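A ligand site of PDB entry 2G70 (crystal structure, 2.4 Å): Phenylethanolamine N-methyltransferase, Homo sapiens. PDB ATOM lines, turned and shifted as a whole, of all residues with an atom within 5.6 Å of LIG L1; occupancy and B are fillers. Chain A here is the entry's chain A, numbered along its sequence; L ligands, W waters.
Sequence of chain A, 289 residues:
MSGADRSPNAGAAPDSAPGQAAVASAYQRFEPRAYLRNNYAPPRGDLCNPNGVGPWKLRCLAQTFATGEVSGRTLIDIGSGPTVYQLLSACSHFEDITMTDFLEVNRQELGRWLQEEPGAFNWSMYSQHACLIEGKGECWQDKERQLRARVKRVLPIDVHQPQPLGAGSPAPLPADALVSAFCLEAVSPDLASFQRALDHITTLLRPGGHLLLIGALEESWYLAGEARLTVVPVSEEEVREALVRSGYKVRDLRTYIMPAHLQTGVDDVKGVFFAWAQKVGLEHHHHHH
OD2 of Asp 267 lies within salt-bridge range of N2 of LIG L1 (3.8 Å).
The side-chain hydroxyl (OH) of Tyr 85 sits at hydrogen-bond distance from an oxygen (O1) of LG2 L2 (3.1 Å).
OH of Tyr 40 lies within hydrogen-bond range of O2 of LG2 L2.
OH of Tyr 35 lies within hydrogen-bond range of O2 of LG2 L2.
The side-chain carboxylate of Glu 219 lies within salt-bridge range of a nitrogen (N2) of LIG L1.
The side-chain amino group of Lys 57 lies within hydrogen-bond range of an oxygen (O3) of LIG L1 (3.4 Å).
The side-chain hydroxyl of Tyr 40 lies close to the side-chain hydroxyl of Tyr 85.
NZ of Lys 57 sits close to OH of Tyr 40, at 3.5 Å.
OD1 of Asn 39 sits at hydrogen-bond distance from NH1 of Arg 44 (2.8 Å).
The side-chain carboxylate (OD1) of Asp 267 is in hydrogen-bond range of the backbone NH (N) of Val 269 (3.1 Å).
The side-chain amino group (NZ) of Lys 57 sits at hydrogen-bond distance from the side-chain hydroxyl (OH) of Tyr 85 (3.3 Å).
The side-chain carboxylate (OD2) of Asp 267 is in salt-bridge range of the guanidinium group (NH1) of Arg 44, 2.9 Å away.
The side-chain amide nitrogen (ND2) of Asn 39 is in hydrogen-bond range of the backbone carbonyl oxygen (O) of Tyr 35.
OH of Tyr 35 touches C1 of LIG L1, 3.0 Å away.
Asn 39 touches LIG L1.
Tyr 40 touches LIG L1.
Arg 44 touches LIG L1.
Val 53 touches LIG L1.
CE1 of Phe 182 touches C7 of LIG L1, at 3.4 Å.
Ala 186 touches LIG L1.
Tyr 222 touches LIG L1 (CD2 to O2, 3.5 Å).
CE of Met 258 touches O1 of LIG L1, at 3.4 Å.
Hydrophobic or aromatic side chains that line LIG L1: Tyr 35, Tyr 40, Val 53, Phe 182, Ala 186, Tyr 222 and Met 258.
Along chain A the residues within 4 Å of LIG L1 span positions 35 to 267.
The nearest printed residue that does not touch LIG L1 is Glu 185 (4.1 Å).
Water W1 bridges an oxygen (O3) of LIG L1 (2.6 Å) and the side-chain amino group (NZ) of Lys 57 (2.7 Å).
Water W2 lies within hydrogen-bond range of the side-chain carboxylate of Asp 267 (2.7 Å), the side-chain amide oxygen of Asn 39 (2.8 Å) and a nitrogen (N2) of LIG L1 (2.9 Å).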
ATOM      1  N   TYR A  35      10.731 -23.118  18.168  1.00  0.00           N
ATOM      2  CA  TYR A  35      11.798 -22.346  18.767  1.00  0.00           C
ATOM      3  C   TYR A  35      12.086 -22.873  20.176  1.00  0.00           C
ATOM      4  O   TYR A  35      13.243 -23.032  20.575  1.00  0.00           O
ATOM      5  CB  TYR A  35      11.399 -20.875  18.840  1.00  0.00           C
ATOM      6  CG  TYR A  35      12.436 -20.019  19.519  1.00  0.00           C
ATOM      7  CD1 TYR A  35      13.550 -19.555  18.828  1.00  0.00           C
ATOM      8  CD2 TYR A  35      12.303 -19.681  20.862  1.00  0.00           C
ATOM      9  CE1 TYR A  35      14.502 -18.790  19.457  1.00  0.00           C
ATOM     10  CE2 TYR A  35      13.247 -18.911  21.494  1.00  0.00           C
ATOM     11  CZ  TYR A  35      14.342 -18.478  20.800  1.00  0.00           C
ATOM     12  OH  TYR A  35      15.282 -17.727  21.455  1.00  0.00           O
ATOM     13  N   ASN A  39      15.677 -24.637  21.470  1.00  0.00           N
ATOM     14  CA  ASN A  39      16.561 -24.001  22.429  1.00  0.00           C
ATOM     15  C   ASN A  39      16.275 -24.254  23.891  1.00  0.00           C
ATOM     16  O   ASN A  39      17.083 -23.913  24.757  1.00  0.00           O
ATOM     17  CB  ASN A  39      16.536 -22.499  22.200  1.00  0.00           C
ATOM     18  CG  ASN A  39      17.044 -22.118  20.841  1.00  0.00           C
ATOM     19  OD1 ASN A  39      18.243 -22.247  20.557  1.00  0.00           O
ATOM     20  ND2 ASN A  39      16.139 -21.638  20.000  1.00  0.00           N
ATOM     21  N   TYR A  40      15.118 -24.827  24.204  1.00  0.00           N
ATOM     22  CA  TYR A  40      14.822 -25.042  25.605  1.00  0.00           C
ATOM     23  C   TYR A  40      14.355 -26.426  25.965  1.00  0.00           C
ATOM     24  O   TYR A  40      13.763 -26.640  27.016  1.00  0.00           O
ATOM     25  CB  TYR A  40      13.866 -23.972  26.083  1.00  0.00           C
ATOM     26  CG  TYR A  40      14.462 -22.602  25.903  1.00  0.00           C
ATOM     27  CD1 TYR A  40      14.259 -21.860  24.744  1.00  0.00           C
ATOM     28  CD2 TYR A  40      15.268 -22.045  26.914  1.00  0.00           C
ATOM     29  CE1 TYR A  40      14.848 -20.607  24.569  1.00  0.00           C
ATOM     30  CE2 TYR A  40      15.860 -20.799  26.759  1.00  0.00           C
ATOM     31  CZ  TYR A  40      15.638 -20.088  25.598  1.00  0.00           C
ATOM     32  OH  TYR A  40      16.236 -18.859  25.456  1.00  0.00           O
ATOM     33  N   ARG A  44      20.089 -28.562  24.882  1.00  0.00           N
ATOM     34  CA  ARG A  44      20.213 -27.202  25.404  1.00  0.00           C
ATOM     35  C   ARG A  44      19.297 -26.942  26.599  1.00  0.00           C
ATOM     36  O   ARG A  44      19.568 -26.099  27.442  1.00  0.00           O
ATOM     37  CB  ARG A  44      19.909 -26.183  24.321  1.00  0.00           C
ATOM     38  CG  ARG A  44      20.887 -26.220  23.167  1.00  0.00           C
ATOM     39  CD  ARG A  44      20.617 -25.091  22.197  1.00  0.00           C
ATOM     40  NE  ARG A  44      21.572 -25.105  21.112  1.00  0.00           N
ATOM     41  CZ  ARG A  44      21.694 -24.151  20.198  1.00  0.00           C
ATOM     42  NH1 ARG A  44      20.910 -23.081  20.238  1.00  0.00           N
ATOM     43  NH2 ARG A  44      22.625 -24.247  19.251  1.00  0.00           N
ATOM     44  N   VAL A  53      24.437 -24.506  28.943  1.00  0.00           N
ATOM     45  CA  VAL A  53      24.157 -23.111  28.690  1.00  0.00           C
ATOM     46  C   VAL A  53      22.983 -22.569  29.544  1.00  0.00           C
ATOM     47  O   VAL A  53      22.966 -21.382  29.895  1.00  0.00           O
ATOM     48  CB  VAL A  53      23.890 -22.918  27.184  1.00  0.00           C
ATOM     49  CG1 VAL A  53      22.708 -23.775  26.746  1.00  0.00           C
ATOM     50  CG2 VAL A  53      23.697 -21.441  26.868  1.00  0.00           C
ATOM     51  N   GLY A  54      22.026 -23.418  29.889  1.00  0.00           N
ATOM     52  CA  GLY A  54      20.915 -22.956  30.711  1.00  0.00           C
ATOM     53  C   GLY A  54      21.367 -22.574  32.115  1.00  0.00           C
ATOM     54  O   GLY A  54      21.031 -21.490  32.634  1.00  0.00           O
ATOM     55  N   LYS A  57      23.210 -19.279  32.065  1.00  0.00           N
ATOM     56  CA  LYS A  57      22.353 -18.113  31.978  1.00  0.00           C
ATOM     57  C   LYS A  57      21.673 -17.833  33.319  1.00  0.00           C
ATOM     58  O   LYS A  57      21.696 -16.699  33.804  1.00  0.00           O
ATOM     59  CB  LYS A  57      21.309 -18.275  30.870  1.00  0.00           C
ATOM     60  CG  LYS A  57      21.771 -17.799  29.493  1.00  0.00           C
ATOM     61  CD  LYS A  57      20.671 -17.947  28.442  1.00  0.00           C
ATOM     62  CE  LYS A  57      20.239 -19.406  28.279  1.00  0.00           C
ATOM     63  NZ  LYS A  57      19.033 -19.587  27.396  1.00  0.00           N
ATOM     64  N   TYR A  85      11.987 -17.912  31.367  1.00  0.00           N
ATOM     65  CA  TYR A  85      13.171 -18.227  32.168  1.00  0.00           C
ATOM     66  C   TYR A  85      14.007 -16.997  32.514  1.00  0.00           C
ATOM     67  O   TYR A  85      14.532 -16.890  33.628  1.00  0.00           O
ATOM     68  CB  TYR A  85      14.064 -19.272  31.437  1.00  0.00           C
ATOM     69  CG  TYR A  85      14.993 -18.671  30.410  1.00  0.00           C
ATOM     70  CD1 TYR A  85      16.210 -18.126  30.785  1.00  0.00           C
ATOM     71  CD2 TYR A  85      14.619 -18.575  29.070  1.00  0.00           C
ATOM     72  CE1 TYR A  85      17.029 -17.484  29.857  1.00  0.00           C
ATOM     73  CE2 TYR A  85      15.426 -17.951  28.138  1.00  0.00           C
ATOM     74  CZ  TYR A  85      16.623 -17.409  28.533  1.00  0.00           C
ATOM     75  OH  TYR A  85      17.412 -16.758  27.608  1.00  0.00           O
ATOM     76  N   PHE A 182      18.536 -12.446  23.720  1.00  0.00           N
ATOM     77  CA  PHE A 182      18.470 -12.931  22.340  1.00  0.00           C
ATOM     78  C   PHE A 182      17.502 -12.145  21.459  1.00  0.00           C
ATOM     79  O   PHE A 182      16.775 -12.746  20.673  1.00  0.00           O
ATOM     80  CB  PHE A 182      18.072 -14.404  22.329  1.00  0.00           C
ATOM     81  CG  PHE A 182      19.065 -15.305  22.996  1.00  0.00           C
ATOM     82  CD1 PHE A 182      18.694 -16.083  24.075  1.00  0.00           C
ATOM     83  CD2 PHE A 182      20.373 -15.354  22.545  1.00  0.00           C
ATOM     84  CE1 PHE A 182      19.629 -16.900  24.712  1.00  0.00           C
ATOM     85  CE2 PHE A 182      21.323 -16.163  23.177  1.00  0.00           C
ATOM     86  CZ  PHE A 182      20.952 -16.942  24.256  1.00  0.00           C
ATOM     87  N   GLU A 185      20.330  -8.516  18.532  1.00  0.00           N
ATOM     88  CA  GLU A 185      21.125  -9.114  17.466  1.00  0.00           C
ATOM     89  C   GLU A 185      20.291  -9.980  16.517  1.00  0.00           C
ATOM     90  O   GLU A 185      20.601 -10.070  15.322  1.00  0.00           O
ATOM     91  CB  GLU A 185      22.285  -9.942  18.035  1.00  0.00           C
ATOM     92  CG  GLU A 185      21.961 -11.389  18.456  1.00  0.00           C
ATOM     93  CD  GLU A 185      21.538 -11.526  19.918  1.00  0.00           C
ATOM     94  OE1 GLU A 185      22.004 -10.711  20.740  1.00  0.00           O
ATOM     95  OE2 GLU A 185      20.750 -12.446  20.241  1.00  0.00           O
ATOM     96  N   ALA A 186      19.237 -10.589  17.040  1.00  0.00           N
ATOM     97  CA  ALA A 186      18.378 -11.468  16.248  1.00  0.00           C
ATOM     98  C   ALA A 186      17.364 -10.732  15.358  1.00  0.00           C
ATOM     99  O   ALA A 186      16.682 -11.362  14.541  1.00  0.00           O
ATOM    100  CB  ALA A 186      17.656 -12.450  17.166  1.00  0.00           C
ATOM    101  N   ALA A 216      23.365 -13.578  21.463  1.00  0.00           N
ATOM    102  CA  ALA A 216      24.174 -14.554  20.725  1.00  0.00           C
ATOM    103  C   ALA A 216      25.520 -13.990  20.274  1.00  0.00           C
ATOM    104  O   ALA A 216      25.633 -12.808  19.978  1.00  0.00           O
ATOM    105  CB  ALA A 216      23.406 -15.052  19.517  1.00  0.00           C
ATOM    106  N   GLU A 219      26.713 -15.340  15.656  1.00  0.00           N
ATOM    107  CA  GLU A 219      25.645 -16.141  15.071  1.00  0.00           C
ATOM    108  C   GLU A 219      25.099 -15.362  13.879  1.00  0.00           C
ATOM    109  O   GLU A 219      24.874 -14.161  13.971  1.00  0.00           O
ATOM    110  CB  GLU A 219      24.514 -16.350  16.071  1.00  0.00           C
ATOM    111  CG  GLU A 219      23.358 -17.186  15.536  1.00  0.00           C
ATOM    112  CD  GLU A 219      22.179 -17.204  16.493  1.00  0.00           C
ATOM    113  OE1 GLU A 219      21.340 -18.127  16.408  1.00  0.00           O
ATOM    114  OE2 GLU A 219      22.075 -16.299  17.344  1.00  0.00           O
ATOM    115  N   TYR A 222      19.392 -18.725  12.522  1.00  0.00           N
ATOM    116  CA  TYR A 222      18.802 -19.738  13.380  1.00  0.00           C
ATOM    117  C   TYR A 222      17.443 -20.111  12.799  1.00  0.00           C
ATOM    118  O   TYR A 222      16.837 -19.314  12.090  1.00  0.00           O
ATOM    119  CB  TYR A 222      18.667 -19.233  14.813  1.00  0.00           C
ATOM    120  CG  TYR A 222      17.563 -18.221  15.046  1.00  0.00           C
ATOM    121  CD1 TYR A 222      16.248 -18.638  15.269  1.00  0.00           C
ATOM    122  CD2 TYR A 222      17.841 -16.858  15.076  1.00  0.00           C
ATOM    123  CE1 TYR A 222      15.249 -17.730  15.523  1.00  0.00           C
ATOM    124  CE2 TYR A 222      16.841 -15.926  15.323  1.00  0.00           C
ATOM    125  CZ  TYR A 222      15.548 -16.371  15.553  1.00  0.00           C
ATOM    126  OH  TYR A 222      14.542 -15.474  15.808  1.00  0.00           O
ATOM    127  N   VAL A 231      20.653 -13.469  11.517  1.00  0.00           N
ATOM    128  CA  VAL A 231      21.141 -12.758  12.678  1.00  0.00           C
ATOM    129  C   VAL A 231      22.368 -11.948  12.301  1.00  0.00           C
ATOM    130  O   VAL A 231      23.040 -12.249  11.311  1.00  0.00           O
ATOM    131  CB  VAL A 231      21.510 -13.740  13.816  1.00  0.00           C
ATOM    132  CG1 VAL A 231      21.701 -12.990  15.136  1.00  0.00           C
ATOM    133  CG2 VAL A 231      20.446 -14.827  13.954  1.00  0.00           C
ATOM    134  N   MET A 258      29.952 -21.868  23.433  1.00  0.00           N
ATOM    135  CA  MET A 258      29.106 -23.004  23.072  1.00  0.00           C
ATOM    136  C   MET A 258      29.898 -24.303  22.824  1.00  0.00           C
ATOM    137  O   MET A 258      30.746 -24.359  21.952  1.00  0.00           O
ATOM    138  CB  MET A 258      28.269 -22.624  21.838  1.00  0.00           C
ATOM    139  CG  MET A 258      26.959 -23.413  21.677  1.00  0.00           C
ATOM    140  SD  MET A 258      25.729 -23.155  23.021  1.00  0.00           S
ATOM    141  CE  MET A 258      25.472 -21.406  22.956  1.00  0.00           C
ATOM    142  N   ASP A 267      21.173 -23.731  14.447  1.00  0.00           N
ATOM    143  CA  ASP A 267      21.788 -22.436  14.205  1.00  0.00           C
ATOM    144  C   ASP A 267      23.288 -22.586  14.081  1.00  0.00           C
ATOM    145  O   ASP A 267      23.792 -23.695  13.938  1.00  0.00           O
ATOM    146  CB  ASP A 267      21.441 -21.443  15.320  1.00  0.00           C
ATOM    147  CG  ASP A 267      21.838 -21.919  16.710  1.00  0.00           C
ATOM    148  OD1 ASP A 267      22.977 -22.410  16.862  1.00  0.00           O
ATOM    149  OD2 ASP A 267      21.030 -21.794  17.648  1.00  0.00           O
ATOM    150  N   VAL A 269      25.381 -20.512  16.219  1.00  0.00           N
ATOM    151  CA  VAL A 269      25.844 -19.689  17.326  1.00  0.00           C
ATOM    152  C   VAL A 269      27.187 -20.208  17.856  1.00  0.00           C
ATOM    153  O   VAL A 269      27.396 -21.419  17.977  1.00  0.00           O
ATOM    154  CB  VAL A 269      24.782 -19.641  18.463  1.00  0.00           C
ATOM    155  CG1 VAL A 269      24.694 -20.990  19.176  1.00  0.00           C
ATOM    156  CG2 VAL A 269      25.109 -18.534  19.434  1.00  0.00           C
ATOM    157  N   VAL A 272      27.462 -17.331  23.914  1.00  0.00           N
ATOM    158  CA  VAL A 272      26.388 -16.533  24.486  1.00  0.00           C
ATOM    159  C   VAL A 272      27.043 -15.530  25.418  1.00  0.00           C
ATOM    160  O   VAL A 272      28.005 -15.867  26.113  1.00  0.00           O
ATOM    161  CB  VAL A 272      25.401 -17.404  25.325  1.00  0.00           C
ATOM    162  CG1 VAL A 272      24.289 -16.538  25.882  1.00  0.00           C
ATOM    163  CG2 VAL A 272      24.820 -18.551  24.466  1.00  0.00           C
HETATM  164  C1  LIG L   1      18.159 -17.947  20.528  1.00  0.00           C
HETATM  165  C2  LIG L   1      19.147 -17.299  19.551  1.00  0.00           C
HETATM  166  O1  LIG L   1      22.182 -21.940  23.716  1.00  0.00           O
HETATM  167  C3  LIG L   1      20.893 -18.985  19.820  1.00  0.00           C
HETATM  168  C4  LIG L   1      20.860 -20.212  22.012  1.00  0.00           C
HETATM  169  C5  LIG L   1      20.274 -20.570  23.219  1.00  0.00           C
HETATM  170  C6  LIG L   1      19.018 -20.079  23.553  1.00  0.00           C
HETATM  171  C7  LIG L   1      18.352 -19.232  22.664  1.00  0.00           C
HETATM  172  O2  LIG L   1      19.356 -15.551  17.899  1.00  0.00           O
HETATM  173  C8  LIG L   1      18.419 -16.419  18.536  1.00  0.00           C
HETATM  174  C9  LIG L   1      18.930 -18.869  21.460  1.00  0.00           C
HETATM  175  N1  LIG L   1      20.892 -21.433  24.033  1.00  0.00           N
HETATM  176  O3  LIG L   1      20.261 -21.864  25.237  1.00  0.00           O
HETATM  177  C10 LIG L   1      20.191 -19.355  21.132  1.00  0.00           C
HETATM  178  N2  LIG L   1      19.945 -18.339  18.889  1.00  0.00           N
HETATM  179  N1  LG2 L   2      13.680 -13.825  24.551  1.00  0.00           N
HETATM  180  C1  LG2 L   2      13.556 -15.214  24.110  1.00  0.00           C
HETATM  181  C2  LG2 L   2      14.715 -16.101  24.603  1.00  0.00           C
HETATM  182  O1  LG2 L   2      15.409 -15.684  25.570  1.00  0.00           O
HETATM  183  O2  LG2 L   2      14.897 -17.208  24.067  1.00  0.00           O
HETATM  184  C3  LG2 L   2      13.387 -15.266  22.569  1.00  0.00           C
HETATM  185  C4  LG2 L   2      14.412 -14.491  21.720  1.00  0.00           C
HETATM  186  S1  LG2 L   2      14.065 -14.589  19.899  1.00  0.00           S
HETATM  187  C5  LG2 L   2      15.403 -15.404  19.075  1.00  0.00           C
HETATM  188  C6  LG2 L   2      13.836 -12.909  19.142  1.00  0.00           C
HETATM  189  C7  LG2 L   2      12.496 -12.250  19.408  1.00  0.00           C
HETATM  190  O3  LG2 L   2      12.413 -10.894  18.886  1.00  0.00           O
HETATM  191  C8  LG2 L   2      11.324 -13.023  18.792  1.00  0.00           C
HETATM  192  O4  LG2 L   2      10.364 -13.341  19.804  1.00  0.00           O
HETATM  193  C9  LG2 L   2      10.765 -12.063  17.739  1.00  0.00           C
HETATM  194  O5  LG2 L   2       9.368 -12.149  17.557  1.00  0.00           O
HETATM  195  C10 LG2 L   2      11.133 -10.705  18.335  1.00  0.00           C
HETATM  196  N2  LG2 L   2      11.176  -9.602  17.364  1.00  0.00           N
HETATM  197  C11 LG2 L   2      11.046  -9.660  15.943  1.00  0.00           C
HETATM  198  N3  LG2 L   2      11.095  -8.481  15.370  1.00  0.00           N
HETATM  199  C12 LG2 L   2      11.266  -7.609  16.434  1.00  0.00           C
HETATM  200  C13 LG2 L   2      11.375  -6.199  16.425  1.00  0.00           C
HETATM  201  N4  LG2 L   2      11.327  -5.454  15.320  1.00  0.00           N
HETATM  202  N5  LG2 L   2      11.527  -5.566  17.627  1.00  0.00           N
HETATM  203  C14 LG2 L   2      11.572  -6.331  18.755  1.00  0.00           C
HETATM  204  N6  LG2 L   2      11.479  -7.678  18.873  1.00  0.00           N
HETATM  205  C15 LG2 L   2      11.319  -8.259  17.662  1.00  0.00           C
HETATM  206  O   HOH W   1      18.793 -22.254  27.368  1.00  0.00           O
HETATM  207  O   HOH W   2      18.634 -20.772  18.168  1.00  0.00           O
